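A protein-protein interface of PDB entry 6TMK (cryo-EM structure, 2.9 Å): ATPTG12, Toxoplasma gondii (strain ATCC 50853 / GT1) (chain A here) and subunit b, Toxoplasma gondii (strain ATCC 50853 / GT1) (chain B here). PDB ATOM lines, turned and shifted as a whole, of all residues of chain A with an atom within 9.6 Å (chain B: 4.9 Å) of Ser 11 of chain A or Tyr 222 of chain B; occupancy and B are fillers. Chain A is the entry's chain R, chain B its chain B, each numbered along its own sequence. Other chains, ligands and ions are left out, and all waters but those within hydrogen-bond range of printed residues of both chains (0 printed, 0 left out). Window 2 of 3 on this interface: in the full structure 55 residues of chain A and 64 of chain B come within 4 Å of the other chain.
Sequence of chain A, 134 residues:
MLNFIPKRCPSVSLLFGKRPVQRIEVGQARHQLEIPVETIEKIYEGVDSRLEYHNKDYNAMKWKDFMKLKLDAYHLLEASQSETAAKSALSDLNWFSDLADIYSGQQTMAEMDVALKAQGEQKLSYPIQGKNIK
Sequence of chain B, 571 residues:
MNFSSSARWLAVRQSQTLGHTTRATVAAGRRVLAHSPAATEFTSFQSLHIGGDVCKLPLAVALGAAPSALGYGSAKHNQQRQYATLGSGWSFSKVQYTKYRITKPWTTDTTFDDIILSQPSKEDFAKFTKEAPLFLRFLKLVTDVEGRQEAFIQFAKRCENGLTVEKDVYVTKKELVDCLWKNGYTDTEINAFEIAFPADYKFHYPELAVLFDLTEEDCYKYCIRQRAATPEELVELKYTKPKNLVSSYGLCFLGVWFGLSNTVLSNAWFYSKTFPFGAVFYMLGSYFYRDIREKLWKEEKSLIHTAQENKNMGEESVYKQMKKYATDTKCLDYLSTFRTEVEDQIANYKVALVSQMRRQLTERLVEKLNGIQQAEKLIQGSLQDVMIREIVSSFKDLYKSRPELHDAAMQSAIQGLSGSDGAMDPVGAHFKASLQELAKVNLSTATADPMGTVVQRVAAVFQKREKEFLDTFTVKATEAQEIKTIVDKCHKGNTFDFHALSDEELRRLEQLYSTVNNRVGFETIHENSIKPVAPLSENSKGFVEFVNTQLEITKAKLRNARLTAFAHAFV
Of the printed residues of chain B, Pro 10 of chain A touches Asp 218. Of chain B, only Asp 218 (3.3 Å), Tyr 222 (3.7 Å) and Arg 225 (3.1 Å) come within 4 Å of Ser 11 of chain A. Of the printed residues of chain B, Leu 14 of chain A touches Cys 179 (3.1 Å) and Tyr 222 (3.9 Å). Of the printed residues of chain B, Asn 55 of chain A touches Arg 225 (3.7 Å). Printed residues of chain B within 4 Å of Asp 57 of chain A: Arg 225 (2.7 Å). Printed residues of chain A within 4 Å of Cys 179 of chain B: Leu 14 (3.1 Å). Of the printed residues of chain A, Asp 218 of chain B touches Pro 10 and Ser 11. Tyr 222 of chain B touches three residues of chain A. The nearest residue of chain B that does not touch Ser 11 of chain A is Lys 221 of chain B (4.1 Å).
OD2 of Asp 57 of chain A lies within salt-bridge range of NH1 of Arg 225 of chain B (2.7 Å). The backbone carbonyl oxygen (O) of Leu 14 of chain A is in hydrogen-bond range of the side-chain sulfur (SG) of Cys 179 of chain B, at 3.1 Å. OD2 of Asp 218 of chain B is in hydrogen-bond range of N of Ser 11 of chain A (3.3 Å). The guanidinium group (NE) of Arg 225 of chain B sits at hydrogen-bond distance from the backbone carbonyl oxygen (O) of Ser 11 of chain A, at 3.1 Å.
Among the printed residues, pairs that only touch across the chains: Pro 10 of chain A with Asp 218 of chain B, Ser 11 of chain A with Tyr 222 of chain B, Val 12 of chain A with Tyr 222 of chain B, Leu 14 of chain A with Tyr 222 of chain B and Asn 55 of chain A with Arg 225 of chain B.
The backbone NH of Lys 7 of chain A sits at hydrogen-bond distance from the backbone carbonyl oxygen of Asp 57 of chain A.
Of the 14 printed residues of chain A, 6 touch a printed residue of chain B. Hydrophobic or aromatic side chains of chain B that line the printed part of chain A: Tyr 222. Along chain B the printed residues that touch a printed residue of chain A span positions 179 to 225. Among the printed residues, 9 pairs touch across the chains. Among the printed residues, Asp or Glu carboxylates within 4 Å of a Lys or Arg side-chain nitrogen of the other chain: Asp 57 of chain A with Arg 225 of chain B.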
ATOM      1  N   PRO A   6     -39.746  13.661  25.169  1.00  0.00           N
ATOM      2  CA  PRO A   6     -38.384  13.637  24.628  1.00  0.00           C
ATOM      3  C   PRO A   6     -38.209  12.534  23.603  1.00  0.00           C
ATOM      4  O   PRO A   6     -38.709  11.420  23.767  1.00  0.00           O
ATOM      5  CB  PRO A   6     -37.514  13.383  25.862  1.00  0.00           C
ATOM      6  CG  PRO A   6     -38.395  13.570  27.025  1.00  0.00           C
ATOM      7  CD  PRO A   6     -39.764  13.266  26.583  1.00  0.00           C
ATOM      8  N   LYS A   7     -37.491  12.856  22.531  1.00  0.00           N
ATOM      9  CA  LYS A   7     -37.118  11.835  21.569  1.00  0.00           C
ATOM     10  C   LYS A   7     -36.259  10.784  22.252  1.00  0.00           C
ATOM     11  O   LYS A   7     -35.348  11.106  23.018  1.00  0.00           O
ATOM     12  CB  LYS A   7     -36.365  12.458  20.400  1.00  0.00           C
ATOM     13  CG  LYS A   7     -37.192  13.398  19.572  1.00  0.00           C
ATOM     14  CD  LYS A   7     -36.534  13.693  18.252  1.00  0.00           C
ATOM     15  CE  LYS A   7     -37.323  14.696  17.451  1.00  0.00           C
ATOM     16  NZ  LYS A   7     -36.761  14.865  16.093  1.00  0.00           N
ATOM     17  N   ARG A   8     -36.556   9.522  21.979  1.00  0.00           N
ATOM     18  CA  ARG A   8     -35.829   8.417  22.579  1.00  0.00           C
ATOM     19  C   ARG A   8     -34.591   8.030  21.783  1.00  0.00           C
ATOM     20  O   ARG A   8     -33.955   7.021  22.101  1.00  0.00           O
ATOM     21  CB  ARG A   8     -36.760   7.219  22.753  1.00  0.00           C
ATOM     22  CG  ARG A   8     -37.419   6.741  21.490  1.00  0.00           C
ATOM     23  CD  ARG A   8     -38.285   5.543  21.773  1.00  0.00           C
ATOM     24  NE  ARG A   8     -39.392   5.426  20.833  1.00  0.00           N
ATOM     25  CZ  ARG A   8     -40.228   4.396  20.793  1.00  0.00           C
ATOM     26  NH1 ARG A   8     -40.079   3.386  21.639  1.00  0.00           N
ATOM     27  NH2 ARG A   8     -41.210   4.377  19.906  1.00  0.00           N
ATOM     28  N   CYS A   9     -34.232   8.810  20.768  1.00  0.00           N
ATOM     29  CA  CYS A   9     -32.981   8.590  20.073  1.00  0.00           C
ATOM     30  C   CYS A   9     -31.803   8.875  21.002  1.00  0.00           C
ATOM     31  O   CYS A   9     -31.887   9.743  21.874  1.00  0.00           O
ATOM     32  CB  CYS A   9     -32.898   9.488  18.846  1.00  0.00           C
ATOM     33  SG  CYS A   9     -34.320   9.372  17.741  1.00  0.00           S
ATOM     34  N   PRO A  10     -30.688   8.160  20.835  1.00  0.00           N
ATOM     35  CA  PRO A  10     -29.554   8.361  21.748  1.00  0.00           C
ATOM     36  C   PRO A  10     -28.871   9.705  21.596  1.00  0.00           C
ATOM     37  O   PRO A  10     -28.195  10.144  22.533  1.00  0.00           O
ATOM     38  CB  PRO A  10     -28.609   7.210  21.389  1.00  0.00           C
ATOM     39  CG  PRO A  10     -28.956   6.857  20.006  1.00  0.00           C
ATOM     40  CD  PRO A  10     -30.415   7.103  19.852  1.00  0.00           C
ATOM     41  N   SER A  11     -29.017  10.373  20.452  1.00  0.00           N
ATOM     42  CA  SER A  11     -28.469  11.711  20.296  1.00  0.00           C
ATOM     43  C   SER A  11     -29.143  12.712  21.221  1.00  0.00           C
ATOM     44  O   SER A  11     -28.560  13.761  21.513  1.00  0.00           O
ATOM     45  CB  SER A  11     -28.605  12.164  18.848  1.00  0.00           C
ATOM     46  OG  SER A  11     -29.907  12.647  18.580  1.00  0.00           O
ATOM     47  N   VAL A  12     -30.352  12.410  21.682  1.00  0.00           N
ATOM     48  CA  VAL A  12     -31.107  13.275  22.579  1.00  0.00           C
ATOM     49  C   VAL A  12     -31.160  12.694  23.983  1.00  0.00           C
ATOM     50  O   VAL A  12     -30.681  13.307  24.938  1.00  0.00           O
ATOM     51  CB  VAL A  12     -32.527  13.527  22.028  1.00  0.00           C
ATOM     52  CG1 VAL A  12     -33.344  14.315  23.021  1.00  0.00           C
ATOM     53  CG2 VAL A  12     -32.461  14.220  20.688  1.00  0.00           C
ATOM     54  N   SER A  13     -31.746  11.512  24.132  1.00  0.00           N
ATOM     55  CA  SER A  13     -31.861  10.830  25.415  1.00  0.00           C
ATOM     56  C   SER A  13     -30.934   9.628  25.343  1.00  0.00           C
ATOM     57  O   SER A  13     -31.325   8.544  24.909  1.00  0.00           O
ATOM     58  CB  SER A  13     -33.287  10.405  25.698  1.00  0.00           C
ATOM     59  OG  SER A  13     -33.608   9.238  24.968  1.00  0.00           O
ATOM     60  N   LEU A  14     -29.695   9.833  25.767  1.00  0.00           N
ATOM     61  CA  LEU A  14     -28.750   8.738  25.872  1.00  0.00           C
ATOM     62  C   LEU A  14     -29.269   7.684  26.840  1.00  0.00           C
ATOM     63  O   LEU A  14     -29.705   8.000  27.950  1.00  0.00           O
ATOM     64  CB  LEU A  14     -27.402   9.277  26.334  1.00  0.00           C
ATOM     65  CG  LEU A  14     -26.145   8.520  25.929  1.00  0.00           C
ATOM     66  CD1 LEU A  14     -25.773   8.785  24.483  1.00  0.00           C
ATOM     67  CD2 LEU A  14     -25.028   8.921  26.846  1.00  0.00           C
ATOM     68  N   LEU A  15     -29.226   6.428  26.405  1.00  0.00           N
ATOM     69  CA  LEU A  15     -29.478   5.276  27.269  1.00  0.00           C
ATOM     70  C   LEU A  15     -30.945   5.154  27.671  1.00  0.00           C
ATOM     71  O   LEU A  15     -31.251   4.862  28.826  1.00  0.00           O
ATOM     72  CB  LEU A  15     -28.612   5.333  28.524  1.00  0.00           C
ATOM     73  CG  LEU A  15     -27.155   5.734  28.385  1.00  0.00           C
ATOM     74  CD1 LEU A  15     -26.636   6.114  29.744  1.00  0.00           C
ATOM     75  CD2 LEU A  15     -26.358   4.615  27.786  1.00  0.00           C
ATOM     76  N   PHE A  16     -31.861   5.357  26.730  1.00  0.00           N
ATOM     77  CA  PHE A  16     -33.273   5.298  27.087  1.00  0.00           C
ATOM     78  C   PHE A  16     -33.681   3.887  27.490  1.00  0.00           C
ATOM     79  O   PHE A  16     -34.076   3.640  28.635  1.00  0.00           O
ATOM     80  CB  PHE A  16     -34.149   5.790  25.945  1.00  0.00           C
ATOM     81  CG  PHE A  16     -35.607   5.605  26.212  1.00  0.00           C
ATOM     82  CD1 PHE A  16     -36.225   6.311  27.221  1.00  0.00           C
ATOM     83  CD2 PHE A  16     -36.355   4.708  25.478  1.00  0.00           C
ATOM     84  CE1 PHE A  16     -37.556   6.137  27.485  1.00  0.00           C
ATOM     85  CE2 PHE A  16     -37.689   4.532  25.740  1.00  0.00           C
ATOM     86  CZ  PHE A  16     -38.290   5.249  26.743  1.00  0.00           C
ATOM     87  N   ASN A  55     -35.501  22.720  20.084  1.00  0.00           N
ATOM     88  CA  ASN A  55     -34.314  22.253  19.376  1.00  0.00           C
ATOM     89  C   ASN A  55     -34.542  20.937  18.652  1.00  0.00           C
ATOM     90  O   ASN A  55     -33.588  20.208  18.372  1.00  0.00           O
ATOM     91  CB  ASN A  55     -33.130  22.118  20.334  1.00  0.00           C
ATOM     92  CG  ASN A  55     -31.799  22.263  19.645  1.00  0.00           C
ATOM     93  OD1 ASN A  55     -31.611  23.129  18.796  1.00  0.00           O
ATOM     94  ND2 ASN A  55     -30.855  21.414  20.019  1.00  0.00           N
ATOM     95  N   LYS A  56     -35.797  20.622  18.341  1.00  0.00           N
ATOM     96  CA  LYS A  56     -36.156  19.362  17.699  1.00  0.00           C
ATOM     97  C   LYS A  56     -35.669  18.179  18.524  1.00  0.00           C
ATOM     98  O   LYS A  56     -35.122  17.207  18.000  1.00  0.00           O
ATOM     99  CB  LYS A  56     -35.624  19.308  16.269  1.00  0.00           C
ATOM    100  CG  LYS A  56     -36.242  20.365  15.384  1.00  0.00           C
ATOM    101  CD  LYS A  56     -35.726  20.297  13.969  1.00  0.00           C
ATOM    102  CE  LYS A  56     -35.948  21.609  13.244  1.00  0.00           C
ATOM    103  NZ  LYS A  56     -37.227  22.260  13.647  1.00  0.00           N
ATOM    104  N   ASP A  57     -35.871  18.276  19.832  1.00  0.00           N
ATOM    105  CA  ASP A  57     -35.566  17.218  20.775  1.00  0.00           C
ATOM    106  C   ASP A  57     -36.805  16.661  21.452  1.00  0.00           C
ATOM    107  O   ASP A  57     -36.715  15.636  22.135  1.00  0.00           O
ATOM    108  CB  ASP A  57     -34.598  17.734  21.843  1.00  0.00           C
ATOM    109  CG  ASP A  57     -33.242  18.092  21.276  1.00  0.00           C
ATOM    110  OD1 ASP A  57     -32.516  18.873  21.923  1.00  0.00           O
ATOM    111  OD2 ASP A  57     -32.899  17.593  20.185  1.00  0.00           O
ATOM    112  N   VAL B 171     -18.936  15.261  28.597  1.00  0.00           N
ATOM    113  CA  VAL B 171     -20.052  15.221  29.528  1.00  0.00           C
ATOM    114  C   VAL B 171     -19.472  15.002  30.914  1.00  0.00           C
ATOM    115  O   VAL B 171     -18.538  14.212  31.088  1.00  0.00           O
ATOM    116  CB  VAL B 171     -21.063  14.114  29.170  1.00  0.00           C
ATOM    117  CG1 VAL B 171     -21.985  13.859  30.313  1.00  0.00           C
ATOM    118  CG2 VAL B 171     -21.870  14.508  27.960  1.00  0.00           C
ATOM    119  N   CYS B 179     -28.097  10.746  34.256  1.00  0.00           N
ATOM    120  CA  CYS B 179     -28.663  10.013  33.131  1.00  0.00           C
ATOM    121  C   CYS B 179     -28.814   8.536  33.464  1.00  0.00           C
ATOM    122  O   CYS B 179     -29.872   7.939  33.232  1.00  0.00           O
ATOM    123  CB  CYS B 179     -27.789  10.190  31.894  1.00  0.00           C
ATOM    124  SG  CYS B 179     -28.563   9.637  30.368  1.00  0.00           S
ATOM    125  N   ASP B 218     -23.693   9.999  17.610  1.00  0.00           N
ATOM    126  CA  ASP B 218     -24.724  10.275  18.602  1.00  0.00           C
ATOM    127  C   ASP B 218     -24.121  10.797  19.898  1.00  0.00           C
ATOM    128  O   ASP B 218     -24.668  11.719  20.518  1.00  0.00           O
ATOM    129  CB  ASP B 218     -25.535   9.008  18.857  1.00  0.00           C
ATOM    130  CG  ASP B 218     -26.463   8.670  17.711  1.00  0.00           C
ATOM    131  OD1 ASP B 218     -26.024   7.974  16.774  1.00  0.00           O
ATOM    132  OD2 ASP B 218     -27.637   9.095  17.747  1.00  0.00           O
ATOM    133  N   CYS B 219     -22.999  10.221  20.331  1.00  0.00           N
ATOM    134  CA  CYS B 219     -22.371  10.695  21.560  1.00  0.00           C
ATOM    135  C   CYS B 219     -21.840  12.113  21.400  1.00  0.00           C
ATOM    136  O   CYS B 219     -21.922  12.923  22.330  1.00  0.00           O
ATOM    137  CB  CYS B 219     -21.260   9.739  21.976  1.00  0.00           C
ATOM    138  SG  CYS B 219     -21.844   8.129  22.515  1.00  0.00           S
ATOM    139  N   TYR B 220     -21.308  12.438  20.221  1.00  0.00           N
ATOM    140  CA  TYR B 220     -20.859  13.793  19.938  1.00  0.00           C
ATOM    141  C   TYR B 220     -22.015  14.774  20.029  1.00  0.00           C
ATOM    142  O   TYR B 220     -21.898  15.841  20.642  1.00  0.00           O
ATOM    143  CB  TYR B 220     -20.218  13.825  18.551  1.00  0.00           C
ATOM    144  CG  TYR B 220     -19.776  15.182  18.067  1.00  0.00           C
ATOM    145  CD1 TYR B 220     -18.533  15.686  18.393  1.00  0.00           C
ATOM    146  CD2 TYR B 220     -20.596  15.949  17.263  1.00  0.00           C
ATOM    147  CE1 TYR B 220     -18.129  16.919  17.948  1.00  0.00           C
ATOM    148  CE2 TYR B 220     -20.200  17.180  16.816  1.00  0.00           C
ATOM    149  CZ  TYR B 220     -18.968  17.662  17.159  1.00  0.00           C
ATOM    150  OH  TYR B 220     -18.579  18.896  16.702  1.00  0.00           O
ATOM    151  N   LYS B 221     -23.142  14.427  19.414  1.00  0.00           N
ATOM    152  CA  LYS B 221     -24.299  15.309  19.448  1.00  0.00           C
ATOM    153  C   LYS B 221     -24.818  15.493  20.868  1.00  0.00           C
ATOM    154  O   LYS B 221     -25.185  16.607  21.266  1.00  0.00           O
ATOM    155  CB  LYS B 221     -25.384  14.750  18.540  1.00  0.00           C
ATOM    156  CG  LYS B 221     -24.993  14.718  17.092  1.00  0.00           C
ATOM    157  CD  LYS B 221     -26.162  14.411  16.203  1.00  0.00           C
ATOM    158  CE  LYS B 221     -25.734  14.279  14.765  1.00  0.00           C
ATOM    159  NZ  LYS B 221     -26.873  13.943  13.877  1.00  0.00           N
ATOM    160  N   TYR B 222     -24.846  14.416  21.652  1.00  0.00           N
ATOM    161  CA  TYR B 222     -25.274  14.525  23.040  1.00  0.00           C
ATOM    162  C   TYR B 222     -24.350  15.445  23.827  1.00  0.00           C
ATOM    163  O   TYR B 222     -24.807  16.317  24.578  1.00  0.00           O
ATOM    164  CB  TYR B 222     -25.327  13.134  23.667  1.00  0.00           C
ATOM    165  CG  TYR B 222     -25.874  13.107  25.069  1.00  0.00           C
ATOM    166  CD1 TYR B 222     -27.232  13.167  25.300  1.00  0.00           C
ATOM    167  CD2 TYR B 222     -25.032  13.022  26.161  1.00  0.00           C
ATOM    168  CE1 TYR B 222     -27.734  13.149  26.573  1.00  0.00           C
ATOM    169  CE2 TYR B 222     -25.528  13.003  27.434  1.00  0.00           C
ATOM    170  CZ  TYR B 222     -26.879  13.067  27.636  1.00  0.00           C
ATOM    171  OH  TYR B 222     -27.375  13.047  28.914  1.00  0.00           O
ATOM    172  N   CYS B 223     -23.040  15.256  23.672  1.00  0.00           N
ATOM    173  CA  CYS B 223     -22.073  16.106  24.354  1.00  0.00           C
ATOM    174  C   CYS B 223     -22.252  17.567  23.968  1.00  0.00           C
ATOM    175  O   CYS B 223     -22.152  18.459  24.816  1.00  0.00           O
ATOM    176  CB  CYS B 223     -20.660  15.632  24.033  1.00  0.00           C
ATOM    177  SG  CYS B 223     -20.166  14.134  24.887  1.00  0.00           S
ATOM    178  N   ILE B 224     -22.513  17.830  22.689  1.00  0.00           N
ATOM    179  CA  ILE B 224     -22.670  19.205  22.230  1.00  0.00           C
ATOM    180  C   ILE B 224     -23.916  19.830  22.833  1.00  0.00           C
ATOM    181  O   ILE B 224     -23.900  20.991  23.256  1.00  0.00           O
ATOM    182  CB  ILE B 224     -22.705  19.251  20.697  1.00  0.00           C
ATOM    183  CG1 ILE B 224     -21.338  18.892  20.131  1.00  0.00           C
ATOM    184  CG2 ILE B 224     -23.118  20.625  20.226  1.00  0.00           C
ATOM    185  CD1 ILE B 224     -20.344  19.987  20.205  1.00  0.00           C
ATOM    186  N   ARG B 225     -25.017  19.082  22.871  1.00  0.00           N
ATOM    187  CA  ARG B 225     -26.229  19.594  23.498  1.00  0.00           C
ATOM    188  C   ARG B 225     -25.993  19.898  24.970  1.00  0.00           C
ATOM    189  O   ARG B 225     -26.450  20.925  25.489  1.00  0.00           O
ATOM    190  CB  ARG B 225     -27.360  18.584  23.332  1.00  0.00           C
ATOM    191  CG  ARG B 225     -27.998  18.581  21.957  1.00  0.00           C
ATOM    192  CD  ARG B 225     -28.955  17.420  21.779  1.00  0.00           C
ATOM    193  NE  ARG B 225     -28.719  16.724  20.518  1.00  0.00           N
ATOM    194  CZ  ARG B 225     -29.399  16.932  19.397  1.00  0.00           C
ATOM    195  NH1 ARG B 225     -30.381  17.814  19.352  1.00  0.00           N
ATOM    196  NH2 ARG B 225     -29.093  16.248  18.310  1.00  0.00           N
ATOM    197  N   GLN B 226     -25.264  19.023  25.658  1.00  0.00           N
ATOM    198  CA  GLN B 226     -25.043  19.222  27.084  1.00  0.00           C
ATOM    199  C   GLN B 226     -24.076  20.365  27.355  1.00  0.00           C
ATOM    200  O   GLN B 226     -24.139  20.987  28.420  1.00  0.00           O
ATOM    201  CB  GLN B 226     -24.524  17.935  27.716  1.00  0.00           C
ATOM    202  CG  GLN B 226     -25.506  16.793  27.663  1.00  0.00           C
ATOM    203  CD  GLN B 226     -26.751  17.049  28.469  1.00  0.00           C
ATOM    204  OE1 GLN B 226     -27.863  16.975  27.952  1.00  0.00           O
ATOM    205  NE2 GLN B 226     -26.573  17.367  29.740  1.00  0.00           N
